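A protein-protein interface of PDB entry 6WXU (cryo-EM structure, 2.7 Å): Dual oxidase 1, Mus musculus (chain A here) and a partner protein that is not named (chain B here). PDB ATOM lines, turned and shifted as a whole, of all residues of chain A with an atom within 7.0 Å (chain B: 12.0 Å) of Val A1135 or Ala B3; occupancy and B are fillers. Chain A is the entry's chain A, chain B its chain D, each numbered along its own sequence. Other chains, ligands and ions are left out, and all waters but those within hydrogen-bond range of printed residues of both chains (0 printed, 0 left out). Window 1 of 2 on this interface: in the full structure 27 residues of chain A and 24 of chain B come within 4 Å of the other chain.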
ATOM      1  N   PHE A 580      -5.206   2.576  11.679  1.00  0.00           N
ATOM      2  CA  PHE A 580      -3.977   1.907  12.096  1.00  0.00           C
ATOM      3  C   PHE A 580      -3.608   2.296  13.521  1.00  0.00           C
ATOM      4  O   PHE A 580      -3.246   1.439  14.337  1.00  0.00           O
ATOM      5  CB  PHE A 580      -2.844   2.252  11.132  1.00  0.00           C
ATOM      6  CG  PHE A 580      -1.722   1.262  11.131  1.00  0.00           C
ATOM      7  CD1 PHE A 580      -1.860   0.049  10.494  1.00  0.00           C
ATOM      8  CD2 PHE A 580      -0.523   1.553  11.742  1.00  0.00           C
ATOM      9  CE1 PHE A 580      -0.833  -0.862  10.481  1.00  0.00           C
ATOM     10  CE2 PHE A 580       0.508   0.645  11.730  1.00  0.00           C
ATOM     11  CZ  PHE A 580       0.351  -0.565  11.098  1.00  0.00           C
ATOM     12  N   THR A1063      12.343  -5.571   1.589  1.00  0.00           N
ATOM     13  CA  THR A1063      11.174  -4.874   2.110  1.00  0.00           C
ATOM     14  C   THR A1063      11.327  -4.600   3.603  1.00  0.00           C
ATOM     15  O   THR A1063      11.319  -3.444   4.034  1.00  0.00           O
ATOM     16  CB  THR A1063       9.913  -5.698   1.842  1.00  0.00           C
ATOM     17  OG1 THR A1063       9.907  -6.128   0.478  1.00  0.00           O
ATOM     18  CG2 THR A1063       8.680  -4.869   2.102  1.00  0.00           C
ATOM     19  N   THR A1064      11.476  -5.656   4.396  1.00  0.00           N
ATOM     20  CA  THR A1064      11.665  -5.549   5.837  1.00  0.00           C
ATOM     21  C   THR A1064      12.933  -6.298   6.203  1.00  0.00           C
ATOM     22  O   THR A1064      13.012  -7.511   6.004  1.00  0.00           O
ATOM     23  CB  THR A1064      10.475  -6.135   6.601  1.00  0.00           C
ATOM     24  OG1 THR A1064      10.434  -7.551   6.400  1.00  0.00           O
ATOM     25  CG2 THR A1064       9.177  -5.548   6.110  1.00  0.00           C
ATOM     26  N   VAL A1066      15.034  -5.279   9.438  1.00  0.00           N
ATOM     27  CA  VAL A1066      15.036  -5.363  10.893  1.00  0.00           C
ATOM     28  C   VAL A1066      13.769  -6.036  11.395  1.00  0.00           C
ATOM     29  O   VAL A1066      13.796  -6.754  12.400  1.00  0.00           O
ATOM     30  CB  VAL A1066      15.213  -3.963  11.503  1.00  0.00           C
ATOM     31  CG1 VAL A1066      15.261  -4.040  13.015  1.00  0.00           C
ATOM     32  CG2 VAL A1066      16.468  -3.320  10.969  1.00  0.00           C
ATOM     33  N   GLY A1067      12.644  -5.833  10.710  1.00  0.00           N
ATOM     34  CA  GLY A1067      11.396  -6.411  11.176  1.00  0.00           C
ATOM     35  C   GLY A1067      11.382  -7.924  11.083  1.00  0.00           C
ATOM     36  O   GLY A1067      10.987  -8.610  12.028  1.00  0.00           O
ATOM     37  N   HIS A1129       7.986  -9.811  19.156  1.00  0.00           N
ATOM     38  CA  HIS A1129       7.391 -10.469  17.998  1.00  0.00           C
ATOM     39  C   HIS A1129       6.218  -9.666  17.452  1.00  0.00           C
ATOM     40  O   HIS A1129       6.141  -9.383  16.249  1.00  0.00           O
ATOM     41  CB  HIS A1129       6.940 -11.870  18.390  1.00  0.00           C
ATOM     42  CG  HIS A1129       6.816 -12.806  17.237  1.00  0.00           C
ATOM     43  ND1 HIS A1129       6.645 -14.160  17.395  1.00  0.00           N
ATOM     44  CD2 HIS A1129       6.856 -12.586  15.905  1.00  0.00           C
ATOM     45  CE1 HIS A1129       6.584 -14.736  16.209  1.00  0.00           C
ATOM     46  NE2 HIS A1129       6.705 -13.802  15.287  1.00  0.00           N
ATOM     47  N   SER A1130       5.284  -9.296  18.326  1.00  0.00           N
ATOM     48  CA  SER A1130       4.118  -8.545  17.891  1.00  0.00           C
ATOM     49  C   SER A1130       4.505  -7.179  17.347  1.00  0.00           C
ATOM     50  O   SER A1130       3.887  -6.688  16.400  1.00  0.00           O
ATOM     51  CB  SER A1130       3.136  -8.401  19.046  1.00  0.00           C
ATOM     52  OG  SER A1130       2.941  -9.648  19.681  1.00  0.00           O
ATOM     53  N   ALA A1131       5.526  -6.546  17.925  1.00  0.00           N
ATOM     54  CA  ALA A1131       5.948  -5.247  17.414  1.00  0.00           C
ATOM     55  C   ALA A1131       6.648  -5.383  16.069  1.00  0.00           C
ATOM     56  O   ALA A1131       6.451  -4.553  15.174  1.00  0.00           O
ATOM     57  CB  ALA A1131       6.855  -4.555  18.424  1.00  0.00           C
ATOM     58  N   GLY A1132       7.463  -6.422  15.904  1.00  0.00           N
ATOM     59  CA  GLY A1132       8.085  -6.657  14.615  1.00  0.00           C
ATOM     60  C   GLY A1132       7.067  -6.880  13.517  1.00  0.00           C
ATOM     61  O   GLY A1132       7.232  -6.395  12.396  1.00  0.00           O
ATOM     62  N   HIS A1133       5.988  -7.595  13.828  1.00  0.00           N
ATOM     63  CA  HIS A1133       4.954  -7.814  12.825  1.00  0.00           C
ATOM     64  C   HIS A1133       4.021  -6.627  12.662  1.00  0.00           C
ATOM     65  O   HIS A1133       3.398  -6.495  11.609  1.00  0.00           O
ATOM     66  CB  HIS A1133       4.158  -9.069  13.152  1.00  0.00           C
ATOM     67  CG  HIS A1133       4.855 -10.325  12.751  1.00  0.00           C
ATOM     68  ND1 HIS A1133       5.175 -10.607  11.443  1.00  0.00           N
ATOM     69  CD2 HIS A1133       5.316 -11.362  13.483  1.00  0.00           C
ATOM     70  CE1 HIS A1133       5.795 -11.769  11.385  1.00  0.00           C
ATOM     71  NE2 HIS A1133       5.895 -12.248  12.609  1.00  0.00           N
ATOM     72  N   VAL A1134       3.913  -5.760  13.665  1.00  0.00           N
ATOM     73  CA  VAL A1134       3.222  -4.496  13.452  1.00  0.00           C
ATOM     74  C   VAL A1134       4.002  -3.625  12.483  1.00  0.00           C
ATOM     75  O   VAL A1134       3.414  -2.883  11.690  1.00  0.00           O
ATOM     76  CB  VAL A1134       2.985  -3.788  14.798  1.00  0.00           C
ATOM     77  CG1 VAL A1134       2.758  -2.308  14.597  1.00  0.00           C
ATOM     78  CG2 VAL A1134       1.800  -4.408  15.506  1.00  0.00           C
ATOM     79  N   VAL A1135       5.332  -3.704  12.513  1.00  0.00           N
ATOM     80  CA  VAL A1135       6.133  -2.964  11.542  1.00  0.00           C
ATOM     81  C   VAL A1135       6.040  -3.610  10.166  1.00  0.00           C
ATOM     82  O   VAL A1135       5.911  -2.918   9.152  1.00  0.00           O
ATOM     83  CB  VAL A1135       7.590  -2.855  12.018  1.00  0.00           C
ATOM     84  CG1 VAL A1135       8.466  -2.332  10.908  1.00  0.00           C
ATOM     85  CG2 VAL A1135       7.676  -1.944  13.219  1.00  0.00           C
ATOM     86  N   ASN A1136       6.105  -4.942  10.106  1.00  0.00           N
ATOM     87  CA  ASN A1136       6.003  -5.637   8.825  1.00  0.00           C
ATOM     88  C   ASN A1136       4.682  -5.341   8.135  1.00  0.00           C
ATOM     89  O   ASN A1136       4.653  -5.005   6.948  1.00  0.00           O
ATOM     90  CB  ASN A1136       6.157  -7.140   9.026  1.00  0.00           C
ATOM     91  CG  ASN A1136       7.542  -7.525   9.437  1.00  0.00           C
ATOM     92  OD1 ASN A1136       8.484  -6.767   9.251  1.00  0.00           O
ATOM     93  ND2 ASN A1136       7.683  -8.716   9.994  1.00  0.00           N
ATOM     94  N   VAL A1137       3.571  -5.474   8.862  1.00  0.00           N
ATOM     95  CA  VAL A1137       2.255  -5.269   8.265  1.00  0.00           C
ATOM     96  C   VAL A1137       2.120  -3.860   7.708  1.00  0.00           C
ATOM     97  O   VAL A1137       1.389  -3.636   6.737  1.00  0.00           O
ATOM     98  CB  VAL A1137       1.158  -5.597   9.295  1.00  0.00           C
ATOM     99  CG1 VAL A1137      -0.183  -5.077   8.850  1.00  0.00           C
ATOM    100  CG2 VAL A1137       1.081  -7.092   9.501  1.00  0.00           C
ATOM    101  N   TYR A1138       2.836  -2.893   8.278  1.00  0.00           N
ATOM    102  CA  TYR A1138       2.805  -1.552   7.708  1.00  0.00           C
ATOM    103  C   TYR A1138       3.566  -1.492   6.394  1.00  0.00           C
ATOM    104  O   TYR A1138       3.103  -0.876   5.431  1.00  0.00           O
ATOM    105  CB  TYR A1138       3.374  -0.537   8.689  1.00  0.00           C
ATOM    106  CG  TYR A1138       3.578   0.819   8.070  1.00  0.00           C
ATOM    107  CD1 TYR A1138       2.514   1.678   7.879  1.00  0.00           C
ATOM    108  CD2 TYR A1138       4.835   1.239   7.670  1.00  0.00           C
ATOM    109  CE1 TYR A1138       2.694   2.915   7.314  1.00  0.00           C
ATOM    110  CE2 TYR A1138       5.022   2.473   7.102  1.00  0.00           C
ATOM    111  CZ  TYR A1138       3.948   3.307   6.927  1.00  0.00           C
ATOM    112  OH  TYR A1138       4.124   4.542   6.362  1.00  0.00           O
ATOM    113  N   LEU A1139       4.738  -2.121   6.331  1.00  0.00           N
ATOM    114  CA  LEU A1139       5.510  -2.127   5.099  1.00  0.00           C
ATOM    115  C   LEU A1139       4.907  -3.037   4.042  1.00  0.00           C
ATOM    116  O   LEU A1139       5.238  -2.893   2.864  1.00  0.00           O
ATOM    117  CB  LEU A1139       6.952  -2.540   5.390  1.00  0.00           C
ATOM    118  CG  LEU A1139       7.709  -1.609   6.336  1.00  0.00           C
ATOM    119  CD1 LEU A1139       9.127  -2.064   6.521  1.00  0.00           C
ATOM    120  CD2 LEU A1139       7.691  -0.194   5.814  1.00  0.00           C
ATOM    121  N   PHE A1140       4.041  -3.972   4.428  1.00  0.00           N
ATOM    122  CA  PHE A1140       3.352  -4.810   3.458  1.00  0.00           C
ATOM    123  C   PHE A1140       2.138  -4.125   2.863  1.00  0.00           C
ATOM    124  O   PHE A1140       1.616  -4.582   1.844  1.00  0.00           O
ATOM    125  CB  PHE A1140       2.903  -6.118   4.102  1.00  0.00           C
ATOM    126  CG  PHE A1140       4.015  -7.070   4.388  1.00  0.00           C
ATOM    127  CD1 PHE A1140       5.226  -6.960   3.740  1.00  0.00           C
ATOM    128  CD2 PHE A1140       3.845  -8.086   5.303  1.00  0.00           C
ATOM    129  CE1 PHE A1140       6.247  -7.846   4.005  1.00  0.00           C
ATOM    130  CE2 PHE A1140       4.861  -8.973   5.570  1.00  0.00           C
ATOM    131  CZ  PHE A1140       6.062  -8.852   4.921  1.00  0.00           C
ATOM    132  N   PHE A1171      -4.560  -8.163   9.692  1.00  0.00           N
ATOM    133  CA  PHE A1171      -4.833  -8.384  11.102  1.00  0.00           C
ATOM    134  C   PHE A1171      -6.083  -9.213  11.340  1.00  0.00           C
ATOM    135  O   PHE A1171      -6.114 -10.021  12.269  1.00  0.00           O
ATOM    136  CB  PHE A1171      -4.970  -7.046  11.824  1.00  0.00           C
ATOM    137  CG  PHE A1171      -3.667  -6.384  12.113  1.00  0.00           C
ATOM    138  CD1 PHE A1171      -2.557  -7.136  12.438  1.00  0.00           C
ATOM    139  CD2 PHE A1171      -3.546  -5.012  12.056  1.00  0.00           C
ATOM    140  CE1 PHE A1171      -1.354  -6.531  12.702  1.00  0.00           C
ATOM    141  CE2 PHE A1171      -2.342  -4.404  12.318  1.00  0.00           C
ATOM    142  CZ  PHE A1171      -1.247  -5.164  12.642  1.00  0.00           C
ATOM    143  N   ALA B   3       9.058   1.444   9.959  1.00  0.00           N
ATOM    144  CA  ALA B   3      10.265   1.998   9.363  1.00  0.00           C
ATOM    145  C   ALA B   3       9.929   3.215   8.520  1.00  0.00           C
ATOM    146  O   ALA B   3       9.182   4.091   8.950  1.00  0.00           O
ATOM    147  CB  ALA B   3      10.978   0.951   8.530  1.00  0.00           C
ATOM    148  N   LEU B   4      10.482   3.267   7.311  1.00  0.00           N
ATOM    149  CA  LEU B   4      10.240   4.396   6.420  1.00  0.00           C
ATOM    150  C   LEU B   4      10.261   3.882   4.989  1.00  0.00           C
ATOM    151  O   LEU B   4      11.300   3.419   4.513  1.00  0.00           O
ATOM    152  CB  LEU B   4      11.282   5.492   6.628  1.00  0.00           C
ATOM    153  CG  LEU B   4      11.217   6.672   5.658  1.00  0.00           C
ATOM    154  CD1 LEU B   4       9.860   7.343   5.733  1.00  0.00           C
ATOM    155  CD2 LEU B   4      12.328   7.666   5.951  1.00  0.00           C
ATOM    156  N   GLY B   5       9.116   3.948   4.318  1.00  0.00           N
ATOM    157  CA  GLY B   5       9.064   3.621   2.910  1.00  0.00           C
ATOM    158  C   GLY B   5       8.870   4.844   2.038  1.00  0.00           C
ATOM    159  O   GLY B   5       7.760   5.369   1.934  1.00  0.00           O
ATOM    160  N   HIS B   6       9.947   5.301   1.400  1.00  0.00           N
ATOM    161  CA  HIS B   6       9.878   6.429   0.483  1.00  0.00           C
ATOM    162  C   HIS B   6      10.587   6.178  -0.836  1.00  0.00           C
ATOM    163  O   HIS B   6      10.464   7.003  -1.748  1.00  0.00           O
ATOM    164  CB  HIS B   6      10.464   7.693   1.133  1.00  0.00           C
ATOM    165  CG  HIS B   6       9.483   8.445   1.978  1.00  0.00           C
ATOM    166  ND1 HIS B   6       9.870   9.329   2.963  1.00  0.00           N
ATOM    167  CD2 HIS B   6       8.130   8.449   1.979  1.00  0.00           C
ATOM    168  CE1 HIS B   6       8.797   9.842   3.536  1.00  0.00           C
ATOM    169  NE2 HIS B   6       7.728   9.326   2.959  1.00  0.00           N
ATOM    170  N   THR B   7      11.312   5.077  -0.970  1.00  0.00           N
ATOM    171  CA  THR B   7      12.004   4.707  -2.191  1.00  0.00           C
ATOM    172  C   THR B   7      11.551   3.312  -2.610  1.00  0.00           C
ATOM    173  O   THR B   7      10.641   2.727  -2.019  1.00  0.00           O
ATOM    174  CB  THR B   7      13.518   4.762  -1.989  1.00  0.00           C
ATOM    175  OG1 THR B   7      13.905   3.767  -1.035  1.00  0.00           O
ATOM    176  CG2 THR B   7      13.940   6.130  -1.475  1.00  0.00           C
ATOM    177  N   PRO B   9      13.853  -0.182  -3.877  1.00  0.00           N
ATOM    178  CA  PRO B   9      13.279  -0.874  -2.721  1.00  0.00           C
ATOM    179  C   PRO B   9      13.361  -0.060  -1.434  1.00  0.00           C
ATOM    180  O   PRO B   9      13.958   1.014  -1.422  1.00  0.00           O
ATOM    181  CB  PRO B   9      14.138  -2.140  -2.604  1.00  0.00           C
ATOM    182  CG  PRO B   9      14.956  -2.196  -3.854  1.00  0.00           C
ATOM    183  CD  PRO B   9      15.130  -0.785  -4.277  1.00  0.00           C
ATOM    184  N   PHE B  10      12.762  -0.576  -0.361  1.00  0.00           N
ATOM    185  CA  PHE B  10      12.776   0.148   0.903  1.00  0.00           C
ATOM    186  C   PHE B  10      14.155   0.097   1.546  1.00  0.00           C
ATOM    187  O   PHE B  10      14.677   1.122   2.001  1.00  0.00           O
ATOM    188  CB  PHE B  10      11.716  -0.419   1.843  1.00  0.00           C
ATOM    189  CG  PHE B  10      10.312  -0.249   1.342  1.00  0.00           C
ATOM    190  CD1 PHE B  10       9.979   0.812   0.521  1.00  0.00           C
ATOM    191  CD2 PHE B  10       9.326  -1.153   1.688  1.00  0.00           C
ATOM    192  CE1 PHE B  10       8.694   0.968   0.061  1.00  0.00           C
ATOM    193  CE2 PHE B  10       8.042  -1.002   1.230  1.00  0.00           C
ATOM    194  CZ  PHE B  10       7.725   0.058   0.416  1.00  0.00           C
ATOM    195  N   TYR B  11      14.761  -1.083   1.594  1.00  0.00           N
ATOM    196  CA  TYR B  11      16.107  -1.255   2.130  1.00  0.00           C
ATOM    197  C   TYR B  11      17.078  -1.293   0.957  1.00  0.00           C
ATOM    198  O   TYR B  11      17.245  -2.328   0.308  1.00  0.00           O
ATOM    199  CB  TYR B  11      16.202  -2.519   2.979  1.00  0.00           C
ATOM    200  CG  TYR B  11      17.621  -2.907   3.321  1.00  0.00           C
ATOM    201  CD1 TYR B  11      18.391  -2.120   4.168  1.00  0.00           C
ATOM    202  CD2 TYR B  11      18.192  -4.060   2.797  1.00  0.00           C
ATOM    203  CE1 TYR B  11      19.687  -2.469   4.479  1.00  0.00           C
ATOM    204  CE2 TYR B  11      19.487  -4.418   3.106  1.00  0.00           C
ATOM    205  CZ  TYR B  11      20.230  -3.619   3.947  1.00  0.00           C
ATOM    206  OH  TYR B  11      21.521  -3.973   4.256  1.00  0.00           O
ATOM    207  N   THR B  12      17.716  -0.159   0.686  1.00  0.00           N
ATOM    208  CA  THR B  12      18.707  -0.043  -0.382  1.00  0.00           C
ATOM    209  C   THR B  12      20.086  -0.163   0.251  1.00  0.00           C
ATOM    210  O   THR B  12      20.631   0.811   0.773  1.00  0.00           O
ATOM    211  CB  THR B  12      18.557   1.275  -1.132  1.00  0.00           C
ATOM    212  OG1 THR B  12      18.650   2.365  -0.207  1.00  0.00           O
ATOM    213  CG2 THR B  12      17.221   1.335  -1.845  1.00  0.00           C
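Among the printed residues, merely in contact across the chains: Leu A1139 with Phe B10, Thr A1063 with Phe B10 and Val A1135 with Ala B3.
Printed residues of chain B within 4 Å of Thr A1063: Phe B10 (3.8 Å). No residue of chain B comes within 4 Å of Val A1066. No residue of chain B comes within 4 Å of Gly A1067. No residue of chain B comes within 4 Å of Gly A1132. Val A1135 touches just one residue of chain B: Ala B3 (3.9 Å). No residue of chain B comes within 4 Å of Asn A1136. No residue of chain B comes within 4 Å of Val A1137. Leu A1139 touches just one residue of chain B: Phe B10. Ala B3 touches just one residue of chain A: Val A1135. Of the printed residues of chain A, Phe B10 touches Thr A1063 (3.8 Å) and Leu A1139 (3.8 Å). The nearest residue of chain B that does not touch Val A1135 is Leu B4 (7.0 Å). The nearest residue of chain A that does not touch Ala B3 is Leu A1139 (4.1 Å). The nearest printed residue of chain A that does not touch Phe B10 is Thr A1064 (5.7 Å).
Of the 9 printed residues of chain B, 2 touch a printed residue of chain A. Hydrophobic or aromatic side chains of chain B that line the printed part of chain A: Phe B10. Hydrophobic or aromatic side chains of chain A that line the printed part of chain B: Val A1135. Among the printed residues, 3 pairs touch across the chains. Among the printed residues, no Asp or Glu carboxylate lies within 4 Å of a Lys or Arg side-chain nitrogen of the other chain.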
